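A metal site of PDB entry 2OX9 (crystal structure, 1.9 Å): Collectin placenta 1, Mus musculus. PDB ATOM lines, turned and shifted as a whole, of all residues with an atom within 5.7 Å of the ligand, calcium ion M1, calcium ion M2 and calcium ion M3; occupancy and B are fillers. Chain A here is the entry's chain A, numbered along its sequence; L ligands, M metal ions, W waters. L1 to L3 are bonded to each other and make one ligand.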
ATOM      1  N   ASP A  68      -4.431  -8.629  25.021  1.00  0.00           N
ATOM      2  CA  ASP A  68      -4.093  -8.469  23.611  1.00  0.00           C
ATOM      3  C   ASP A  68      -3.964  -6.969  23.332  1.00  0.00           C
ATOM      4  O   ASP A  68      -4.341  -6.483  22.265  1.00  0.00           O
ATOM      5  CB  ASP A  68      -5.154  -9.138  22.703  1.00  0.00           C
ATOM      6  CG  ASP A  68      -6.455  -8.354  22.641  1.00  0.00           C
ATOM      7  OD1 ASP A  68      -6.763  -7.615  23.581  1.00  0.00           O
ATOM      8  OD2 ASP A  68      -7.182  -8.497  21.628  1.00  0.00           O
ATOM      9  N   SER A  69      -3.425  -6.259  24.317  1.00  0.00           N
ATOM     10  CA  SER A  69      -3.206  -4.814  24.230  1.00  0.00           C
ATOM     11  C   SER A  69      -2.052  -4.479  23.293  1.00  0.00           C
ATOM     12  O   SER A  69      -2.097  -3.471  22.596  1.00  0.00           O
ATOM     13  CB  SER A  69      -2.898  -4.233  25.608  1.00  0.00           C
ATOM     14  OG  SER A  69      -3.988  -4.379  26.499  1.00  0.00           O
ATOM     15  N   GLU A  72      -3.954  -6.170  18.920  1.00  0.00           N
ATOM     16  CA  GLU A  72      -5.308  -6.706  18.908  1.00  0.00           C
ATOM     17  C   GLU A  72      -5.369  -8.126  18.328  1.00  0.00           C
ATOM     18  O   GLU A  72      -4.786  -8.402  17.276  1.00  0.00           O
ATOM     19  CB  GLU A  72      -6.230  -5.766  18.130  1.00  0.00           C
ATOM     20  CG  GLU A  72      -7.708  -6.128  18.137  1.00  0.00           C
ATOM     21  CD  GLU A  72      -8.284  -6.230  19.542  1.00  0.00           C
ATOM     22  OE1 GLU A  72      -7.900  -5.404  20.394  1.00  0.00           O
ATOM     23  OE2 GLU A  72      -9.118  -7.113  19.787  1.00  0.00           O
ATOM     24  N   SER A  73      -6.071  -9.009  19.031  1.00  0.00           N
ATOM     25  CA  SER A  73      -6.256 -10.407  18.644  1.00  0.00           C
ATOM     26  C   SER A  73      -5.078 -11.330  18.884  1.00  0.00           C
ATOM     27  O   SER A  73      -5.172 -12.534  18.672  1.00  0.00           O
ATOM     28  CB  SER A  73      -6.699 -10.517  17.180  1.00  0.00           C
ATOM     29  OG  SER A  73      -8.038 -10.077  17.036  1.00  0.00           O
ATOM     30  N   TRP A  75      -3.338 -12.674  21.673  1.00  0.00           N
ATOM     31  CA  TRP A  75      -3.392 -12.892  23.110  1.00  0.00           C
ATOM     32  C   TRP A  75      -2.160 -13.569  23.697  1.00  0.00           C
ATOM     33  O   TRP A  75      -1.727 -14.599  23.198  1.00  0.00           O
ATOM     34  CB  TRP A  75      -4.654 -13.686  23.472  1.00  0.00           C
ATOM     35  CG  TRP A  75      -5.918 -12.917  23.246  1.00  0.00           C
ATOM     36  CD1 TRP A  75      -6.623 -12.829  22.076  1.00  0.00           C
ATOM     37  CD2 TRP A  75      -6.600 -12.090  24.191  1.00  0.00           C
ATOM     38  NE1 TRP A  75      -7.704 -11.998  22.252  1.00  0.00           N
ATOM     39  CE2 TRP A  75      -7.713 -11.530  23.539  1.00  0.00           C
ATOM     40  CE3 TRP A  75      -6.367 -11.763  25.542  1.00  0.00           C
ATOM     41  CZ2 TRP A  75      -8.607 -10.667  24.179  1.00  0.00           C
ATOM     42  CZ3 TRP A  75      -7.258 -10.907  26.175  1.00  0.00           C
ATOM     43  CH2 TRP A  75      -8.359 -10.358  25.494  1.00  0.00           C
ATOM     44  N   LYS A  89     -15.364 -18.548  25.801  1.00  0.00           N
ATOM     45  CA  LYS A  89     -16.746 -18.934  25.649  1.00  0.00           C
ATOM     46  C   LYS A  89     -16.981 -18.753  24.146  1.00  0.00           C
ATOM     47  O   LYS A  89     -16.311 -17.935  23.512  1.00  0.00           O
ATOM     48  CB  LYS A  89     -17.652 -17.974  26.441  1.00  0.00           C
ATOM     49  CG  LYS A  89     -19.149 -18.176  26.195  1.00  0.00           C
ATOM     50  CD  LYS A  89     -19.964 -17.149  26.945  1.00  0.00           C
ATOM     51  CE  LYS A  89     -21.453 -17.294  26.657  1.00  0.00           C
ATOM     52  NZ  LYS A  89     -22.228 -16.240  27.351  1.00  0.00           N
ATOM     53  N   ALA A  90     -17.906 -19.515  23.568  1.00  0.00           N
ATOM     54  CA  ALA A  90     -18.173 -19.417  22.137  1.00  0.00           C
ATOM     55  C   ALA A  90     -18.595 -17.986  21.778  1.00  0.00           C
ATOM     56  O   ALA A  90     -19.473 -17.421  22.420  1.00  0.00           O
ATOM     57  CB  ALA A  90     -19.257 -20.408  21.738  1.00  0.00           C
ATOM     58  N   GLN A  92     -16.578 -15.459  21.918  1.00  0.00           N
ATOM     59  CA  GLN A  92     -15.563 -14.601  22.514  1.00  0.00           C
ATOM     60  C   GLN A  92     -14.190 -15.048  22.012  1.00  0.00           C
ATOM     61  O   GLN A  92     -14.002 -16.203  21.667  1.00  0.00           O
ATOM     62  CB  GLN A  92     -15.608 -14.710  24.039  1.00  0.00           C
ATOM     63  CG  GLN A  92     -16.902 -14.243  24.633  1.00  0.00           C
ATOM     64  CD  GLN A  92     -17.301 -12.883  24.101  1.00  0.00           C
ATOM     65  OE1 GLN A  92     -16.569 -11.907  24.244  1.00  0.00           O
ATOM     66  NE2 GLN A  92     -18.473 -12.821  23.471  1.00  0.00           N
ATOM     67  N   PRO A  93     -13.210 -14.124  21.960  1.00  0.00           N
ATOM     68  CA  PRO A  93     -13.271 -12.700  22.327  1.00  0.00           C
ATOM     69  C   PRO A  93     -13.964 -11.886  21.241  1.00  0.00           C
ATOM     70  O   PRO A  93     -13.774 -12.140  20.057  1.00  0.00           O
ATOM     71  CB  PRO A  93     -11.798 -12.324  22.501  1.00  0.00           C
ATOM     72  CG  PRO A  93     -11.104 -13.232  21.526  1.00  0.00           C
ATOM     73  CD  PRO A  93     -11.810 -14.536  21.709  1.00  0.00           C
ATOM     74  N   ASP A  94     -14.783 -10.916  21.636  1.00  0.00           N
ATOM     75  CA  ASP A  94     -15.508 -10.122  20.646  1.00  0.00           C
ATOM     76  C   ASP A  94     -15.048  -8.673  20.516  1.00  0.00           C
ATOM     77  O   ASP A  94     -15.538  -7.952  19.651  1.00  0.00           O
ATOM     78  CB  ASP A  94     -17.007 -10.183  20.936  1.00  0.00           C
ATOM     79  CG  ASP A  94     -17.369  -9.608  22.295  1.00  0.00           C
ATOM     80  OD1 ASP A  94     -16.449  -9.275  23.064  1.00  0.00           O
ATOM     81  OD2 ASP A  94     -18.580  -9.484  22.588  1.00  0.00           O
ATOM     82  N   ASN A  95     -14.125  -8.254  21.377  1.00  0.00           N
ATOM     83  CA  ASN A  95     -13.592  -6.887  21.366  1.00  0.00           C
ATOM     84  C   ASN A  95     -14.729  -5.861  21.296  1.00  0.00           C
ATOM     85  O   ASN A  95     -14.662  -4.887  20.549  1.00  0.00           O
ATOM     86  CB  ASN A  95     -12.655  -6.722  20.156  1.00  0.00           C
ATOM     87  CG  ASN A  95     -11.571  -5.678  20.391  1.00  0.00           C
ATOM     88  OD1 ASN A  95     -10.910  -5.672  21.442  1.00  0.00           O
ATOM     89  ND2 ASN A  95     -11.374  -4.803  19.414  1.00  0.00           N
ATOM     90  N   TRP A  96     -15.756  -6.080  22.094  1.00  0.00           N
ATOM     91  CA  TRP A  96     -16.931  -5.212  22.141  1.00  0.00           C
ATOM     92  C   TRP A  96     -16.556  -3.741  22.328  1.00  0.00           C
ATOM     93  O   TRP A  96     -15.719  -3.407  23.162  1.00  0.00           O
ATOM     94  CB  TRP A  96     -17.849  -5.659  23.276  1.00  0.00           C
ATOM     95  CG  TRP A  96     -19.275  -5.259  23.132  1.00  0.00           C
ATOM     96  CD1 TRP A  96     -19.967  -4.395  23.926  1.00  0.00           C
ATOM     97  CD2 TRP A  96     -20.210  -5.747  22.154  1.00  0.00           C
ATOM     98  NE1 TRP A  96     -21.281  -4.315  23.501  1.00  0.00           N
ATOM     99  CE2 TRP A  96     -21.450  -5.131  22.419  1.00  0.00           C
ATOM    100  CE3 TRP A  96     -20.115  -6.637  21.076  1.00  0.00           C
ATOM    101  CZ2 TRP A  96     -22.591  -5.390  21.654  1.00  0.00           C
ATOM    102  CZ3 TRP A  96     -21.248  -6.891  20.308  1.00  0.00           C
ATOM    103  CH2 TRP A  96     -22.473  -6.262  20.612  1.00  0.00           C
ATOM    104  N   PRO A 102     -10.489   1.297  22.434  1.00  0.00           N
ATOM    105  CA  PRO A 102      -9.583   0.163  22.251  1.00  0.00           C
ATOM    106  C   PRO A 102     -10.244  -1.211  22.330  1.00  0.00           C
ATOM    107  O   PRO A 102      -9.595  -2.239  22.114  1.00  0.00           O
ATOM    108  CB  PRO A 102      -8.553   0.373  23.366  1.00  0.00           C
ATOM    109  CG  PRO A 102      -9.400   0.948  24.453  1.00  0.00           C
ATOM    110  CD  PRO A 102     -10.267   1.959  23.732  1.00  0.00           C
ATOM    111  N   GLY A 103     -11.543  -1.215  22.655  1.00  0.00           N
ATOM    112  CA  GLY A 103     -12.269  -2.459  22.750  1.00  0.00           C
ATOM    113  C   GLY A 103     -12.059  -3.185  24.067  1.00  0.00           C
ATOM    114  O   GLY A 103     -12.044  -2.567  25.132  1.00  0.00           O
ATOM    115  N   GLU A 104     -11.887  -4.499  23.988  1.00  0.00           N
ATOM    116  CA  GLU A 104     -11.669  -5.342  25.171  1.00  0.00           C
ATOM    117  C   GLU A 104     -10.340  -6.047  24.980  1.00  0.00           C
ATOM    118  O   GLU A 104     -10.191  -6.894  24.096  1.00  0.00           O
ATOM    119  CB  GLU A 104     -12.812  -6.359  25.305  1.00  0.00           C
ATOM    120  CG  GLU A 104     -14.194  -5.691  25.403  1.00  0.00           C
ATOM    121  CD  GLU A 104     -15.316  -6.666  25.702  1.00  0.00           C
ATOM    122  OE1 GLU A 104     -15.580  -7.559  24.870  1.00  0.00           O
ATOM    123  OE2 GLU A 104     -15.942  -6.547  26.775  1.00  0.00           O
ATOM    124  N   ASP A 105      -9.372  -5.727  25.830  1.00  0.00           N
ATOM    125  CA  ASP A 105      -8.055  -6.305  25.697  1.00  0.00           C
ATOM    126  C   ASP A 105      -7.542  -7.034  26.946  1.00  0.00           C
ATOM    127  O   ASP A 105      -6.345  -7.335  27.046  1.00  0.00           O
ATOM    128  CB  ASP A 105      -7.054  -5.203  25.317  1.00  0.00           C
ATOM    129  CG  ASP A 105      -7.455  -4.461  24.046  1.00  0.00           C
ATOM    130  OD1 ASP A 105      -8.409  -4.903  23.361  1.00  0.00           O
ATOM    131  OD2 ASP A 105      -6.812  -3.434  23.742  1.00  0.00           O
ATOM    132  N   ILE A 110     -15.592 -16.061  33.519  1.00  0.00           N
ATOM    133  CA  ILE A 110     -16.994 -15.783  33.773  1.00  0.00           C
ATOM    134  C   ILE A 110     -17.724 -17.078  34.149  1.00  0.00           C
ATOM    135  O   ILE A 110     -17.124 -17.969  34.755  1.00  0.00           O
ATOM    136  CB  ILE A 110     -17.673 -15.117  32.543  1.00  0.00           C
ATOM    137  CG1 ILE A 110     -17.375 -15.924  31.290  1.00  0.00           C
ATOM    138  CG2 ILE A 110     -17.181 -13.680  32.409  1.00  0.00           C
ATOM    139  CD1 ILE A 110     -18.090 -15.401  30.056  1.00  0.00           C
ATOM    140  N   ASN A 116     -13.675 -14.603  28.838  1.00  0.00           N
ATOM    141  CA  ASN A 116     -14.299 -13.513  28.133  1.00  0.00           C
ATOM    142  C   ASN A 116     -13.352 -12.325  28.155  1.00  0.00           C
ATOM    143  O   ASN A 116     -12.588 -12.157  29.099  1.00  0.00           O
ATOM    144  CB  ASN A 116     -15.610 -13.117  28.795  1.00  0.00           C
ATOM    145  CG  ASN A 116     -16.145 -11.817  28.261  1.00  0.00           C
ATOM    146  OD1 ASN A 116     -16.291 -11.651  27.045  1.00  0.00           O
ATOM    147  ND2 ASN A 116     -16.443 -10.886  29.156  1.00  0.00           N
ATOM    148  N   ASP A 117     -13.390 -11.508  27.112  1.00  0.00           N
ATOM    149  CA  ASP A 117     -12.545 -10.331  27.067  1.00  0.00           C
ATOM    150  C   ASP A 117     -13.355  -9.151  27.582  1.00  0.00           C
ATOM    151  O   ASP A 117     -14.527  -8.978  27.217  1.00  0.00           O
ATOM    152  CB  ASP A 117     -12.037 -10.088  25.618  1.00  0.00           C
ATOM    153  CG  ASP A 117     -13.160 -10.017  24.592  1.00  0.00           C
ATOM    154  OD1 ASP A 117     -14.229 -10.636  24.800  1.00  0.00           O
ATOM    155  OD2 ASP A 117     -12.968  -9.354  23.545  1.00  0.00           O
ATOM    156  N   PHE A 118     -12.755  -8.372  28.478  1.00  0.00           N
ATOM    157  CA  PHE A 118     -13.414  -7.208  29.065  1.00  0.00           C
ATOM    158  C   PHE A 118     -12.590  -5.961  28.754  1.00  0.00           C
ATOM    159  O   PHE A 118     -11.420  -6.049  28.375  1.00  0.00           O
ATOM    160  CB  PHE A 118     -13.474  -7.274  30.598  1.00  0.00           C
ATOM    161  CG  PHE A 118     -14.169  -8.489  31.150  1.00  0.00           C
ATOM    162  CD1 PHE A 118     -13.488  -9.689  31.282  1.00  0.00           C
ATOM    163  CD2 PHE A 118     -15.464  -8.392  31.645  1.00  0.00           C
ATOM    164  CE1 PHE A 118     -14.088 -10.784  31.889  1.00  0.00           C
ATOM    165  CE2 PHE A 118     -16.074  -9.486  32.262  1.00  0.00           C
ATOM    166  CZ  PHE A 118     -15.382 -10.688  32.384  1.00  0.00           C
HETATM  167  C1  LIG L   1     -23.414 -12.654  27.436  1.00  0.00           C
HETATM  168  C2  LIG L   1     -23.806 -13.122  26.022  1.00  0.00           C
HETATM  169  C3  LIG L   1     -22.811 -12.574  25.001  1.00  0.00           C
HETATM  170  C4  LIG L   1     -21.391 -12.966  25.392  1.00  0.00           C
HETATM  171  C5  LIG L   1     -21.087 -12.466  26.808  1.00  0.00           C
HETATM  172  C6  LIG L   1     -19.700 -12.897  27.286  1.00  0.00           C
HETATM  173  O1  LIG L   1     -25.109 -12.664  25.708  1.00  0.00           O
HETATM  174  O2  LIG L   1     -23.121 -13.081  23.712  1.00  0.00           O
HETATM  175  O3  LIG L   1     -21.254 -14.378  25.338  1.00  0.00           O
HETATM  176  O4  LIG L   1     -22.060 -12.993  27.741  1.00  0.00           O
HETATM  177  C1  LG2 L   2     -25.236  -9.890  30.705  1.00  0.00           C
HETATM  178  C2  LG2 L   2     -25.180 -10.488  29.302  1.00  0.00           C
HETATM  179  C3  LG2 L   2     -23.737 -10.803  28.924  1.00  0.00           C
HETATM  180  C4  LG2 L   2     -22.885  -9.541  29.065  1.00  0.00           C
HETATM  181  C5  LG2 L   2     -23.031  -8.976  30.475  1.00  0.00           C
HETATM  182  C6  LG2 L   2     -22.292  -7.655  30.640  1.00  0.00           C
HETATM  183  C7  LG2 L   2     -26.815 -11.889  28.222  1.00  0.00           C
HETATM  184  C8  LG2 L   2     -27.929 -12.899  28.423  1.00  0.00           C
HETATM  185  N1  LG2 L   2     -25.995 -11.692  29.253  1.00  0.00           N
HETATM  186  O1  LG2 L   2     -26.541  -9.536  31.001  1.00  0.00           O
HETATM  187  O2  LG2 L   2     -23.673 -11.286  27.571  1.00  0.00           O
HETATM  188  O3  LG2 L   2     -21.505  -9.845  28.798  1.00  0.00           O
HETATM  189  O4  LG2 L   2     -24.428  -8.710  30.760  1.00  0.00           O
HETATM  190  O5  LG2 L   2     -22.709  -6.714  29.671  1.00  0.00           O
HETATM  191  O6  LG2 L   2     -26.691 -11.307  27.137  1.00  0.00           O
HETATM  192  C1  LG3 L   3     -20.838  -8.979  27.943  1.00  0.00           C
HETATM  193  C2  LG3 L   3     -19.331  -9.191  28.096  1.00  0.00           C
HETATM  194  C3  LG3 L   3     -18.568  -8.331  27.080  1.00  0.00           C
HETATM  195  C4  LG3 L   3     -19.109  -8.548  25.668  1.00  0.00           C
HETATM  196  C5  LG3 L   3     -20.631  -8.385  25.636  1.00  0.00           C
HETATM  197  C6  LG3 L   3     -21.230  -8.724  24.279  1.00  0.00           C
HETATM  198  O1  LG3 L   3     -18.936  -8.841  29.407  1.00  0.00           O
HETATM  199  O2  LG3 L   3     -17.198  -8.680  27.129  1.00  0.00           O
HETATM  200  O3  LG3 L   3     -18.754  -9.849  25.219  1.00  0.00           O
HETATM  201  O4  LG3 L   3     -21.253  -9.265  26.602  1.00  0.00           O
HETATM  202  O5  LG3 L   3     -22.563  -8.260  24.173  1.00  0.00           O
HETATM  203 CA    CA M   1     -16.064  -9.849  25.460  1.00  0.00          CA
HETATM  204 CA    CA M   2      -8.939  -6.935  22.167  1.00  0.00          CA
HETATM  205 CA    CA M   3      -7.618  -3.429  21.562  1.00  0.00          CA
HETATM  206  O   HOH W   1     -20.508 -14.718  23.014  1.00  0.00           O
HETATM  207  O   HOH W   2     -23.480 -16.052  23.369  1.00  0.00           O
HETATM  208  O   HOH W   3     -21.551 -13.854  20.812  1.00  0.00           O
HETATM  209  O   HOH W   4      -5.667  -4.092  21.071  1.00  0.00           O
HETATM  210  O   HOH W   5     -24.451 -11.723  21.527  1.00  0.00           O
HETATM  211  O   HOH W   6     -10.940  -8.629  21.892  1.00  0.00           O
HETATM  212  O   HOH W   7     -21.446 -12.879  31.108  1.00  0.00           O
HETATM  213  O   HOH W   8     -18.366  -6.467  30.064  1.00  0.00           O
HETATM  214  O   HOH W   9     -19.424 -10.810  30.952  1.00  0.00           O
HETATM  215  O   HOH W  10      -8.567  -2.671  19.363  1.00  0.00           O
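An oxygen (O3) of LIG L1 lies within hydrogen-bond range of the side-chain amino group (NZ) of Lys 89, at 2.9 Å.
OD1 of Asp 117 binds calcium ion M1 (2.1 Å).
Calcium ion M1 is bound by O2 of LG3 L3.
The side-chain amide oxygen (OD1) of Asn 116 binds calcium ion M1 (2.4 Å).
OE1 of Glu 104 is bound to calcium ion M1, at 2.4 Å.
Calcium ion M1 is bound by OE1 of Gln 92, 2.4 Å away.
O of Asp 117 binds calcium ion M1, 2.5 Å away.
Calcium ion M1 is bound by OD1 of Asp 94.
An oxygen (O3) of LG3 L3 binds calcium ion M1 (2.7 Å).
Calcium ion M1 has eight donor atoms within binding distance.
The side-chain carboxylate (OD2) of Asp 117 lies within hydrogen-bond range of the backbone NH (N) of Asn 95 (2.7 Å).
OE1 of Glu 104 lies close to N of Trp 96 (3.2 Å).
The backbone NH (N) of Asp 105 sits at hydrogen-bond distance from the backbone carbonyl oxygen (O) of Phe 118, 3.3 Å away.
The side-chain carboxylate of Asp 68 lies close to the backbone NH of Ser 73 (2.9 Å).
OD1 of Asp 94 sits close to N of Trp 96.
Water W6 lies within hydrogen-bond range of OD2 of Asp 117 (2.7 Å) and N of Asn 95 (3.2 Å).
Water W1 lies within hydrogen-bond range of O3 of LIG L1 (2.5 Å), NE2 of Gln 92 (2.8 Å) and O of Ala 90 (3.0 Å).
Water W9 bridges O1 of LG3 L3 and ND2 of Asn 116.
Within 4 Å of calcium ion M2: Asp 68, Glu 72, Asn 95, Glu 104 and Asp 105.
Along chain A the residues within 4 Å of calcium ion M2 span positions 68 to 105.
The nearest printed residue that does not touch calcium ion M2 is Trp 75 (4.3 Å).
Merely in contact with the ligand: Trp 96 (3.8 Å).
Seven residues have an atom within 4 Å of the ligand: Lys 89, Gln 92, Asp 94, Trp 96, Glu 104, Asn 116 and Asp 117.
The nearest printed residue that does not touch the ligand is Ile 110 (4.1 Å).
O of Glu 104 is bound to calcium ion M2.
Calcium ion M2 is bound by OE2 of Glu 72, 2.4 Å away.
OD2 of Asp 68 is bound to calcium ion M2, at 2.4 Å.
Calcium ion M2 is bound by OD1 of Asp 105 (2.4 Å).
OD1 of Asn 95 binds calcium ion M2.
OE1 of Glu 72 is bound to calcium ion M2, at 2.6 Å.
Water W6 binds calcium ion M2 (2.6 Å).
OD1 of Asp 68 binds calcium ion M2.
Water W4 is bound to calcium ion M3 (2.1 Å).
Calcium ion M3 is bound by the side-chain carboxylate (OE1) of Glu 72 (2.3 Å).
Calcium ion M3 is bound by OD2 of Asp 105 (2.3 Å).
O of Pro 102 is bound to calcium ion M3.
The side-chain carboxylate (OD1) of Asp 105 is bound to calcium ion M3 (2.5 Å).
Calcium ion M3 is bound by water W10 (2.5 Å).
Calcium ion M3 has six donor atoms within binding distance.
The nearest printed residue that does not touch calcium ion M1 is Phe 118 (4.7 Å).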
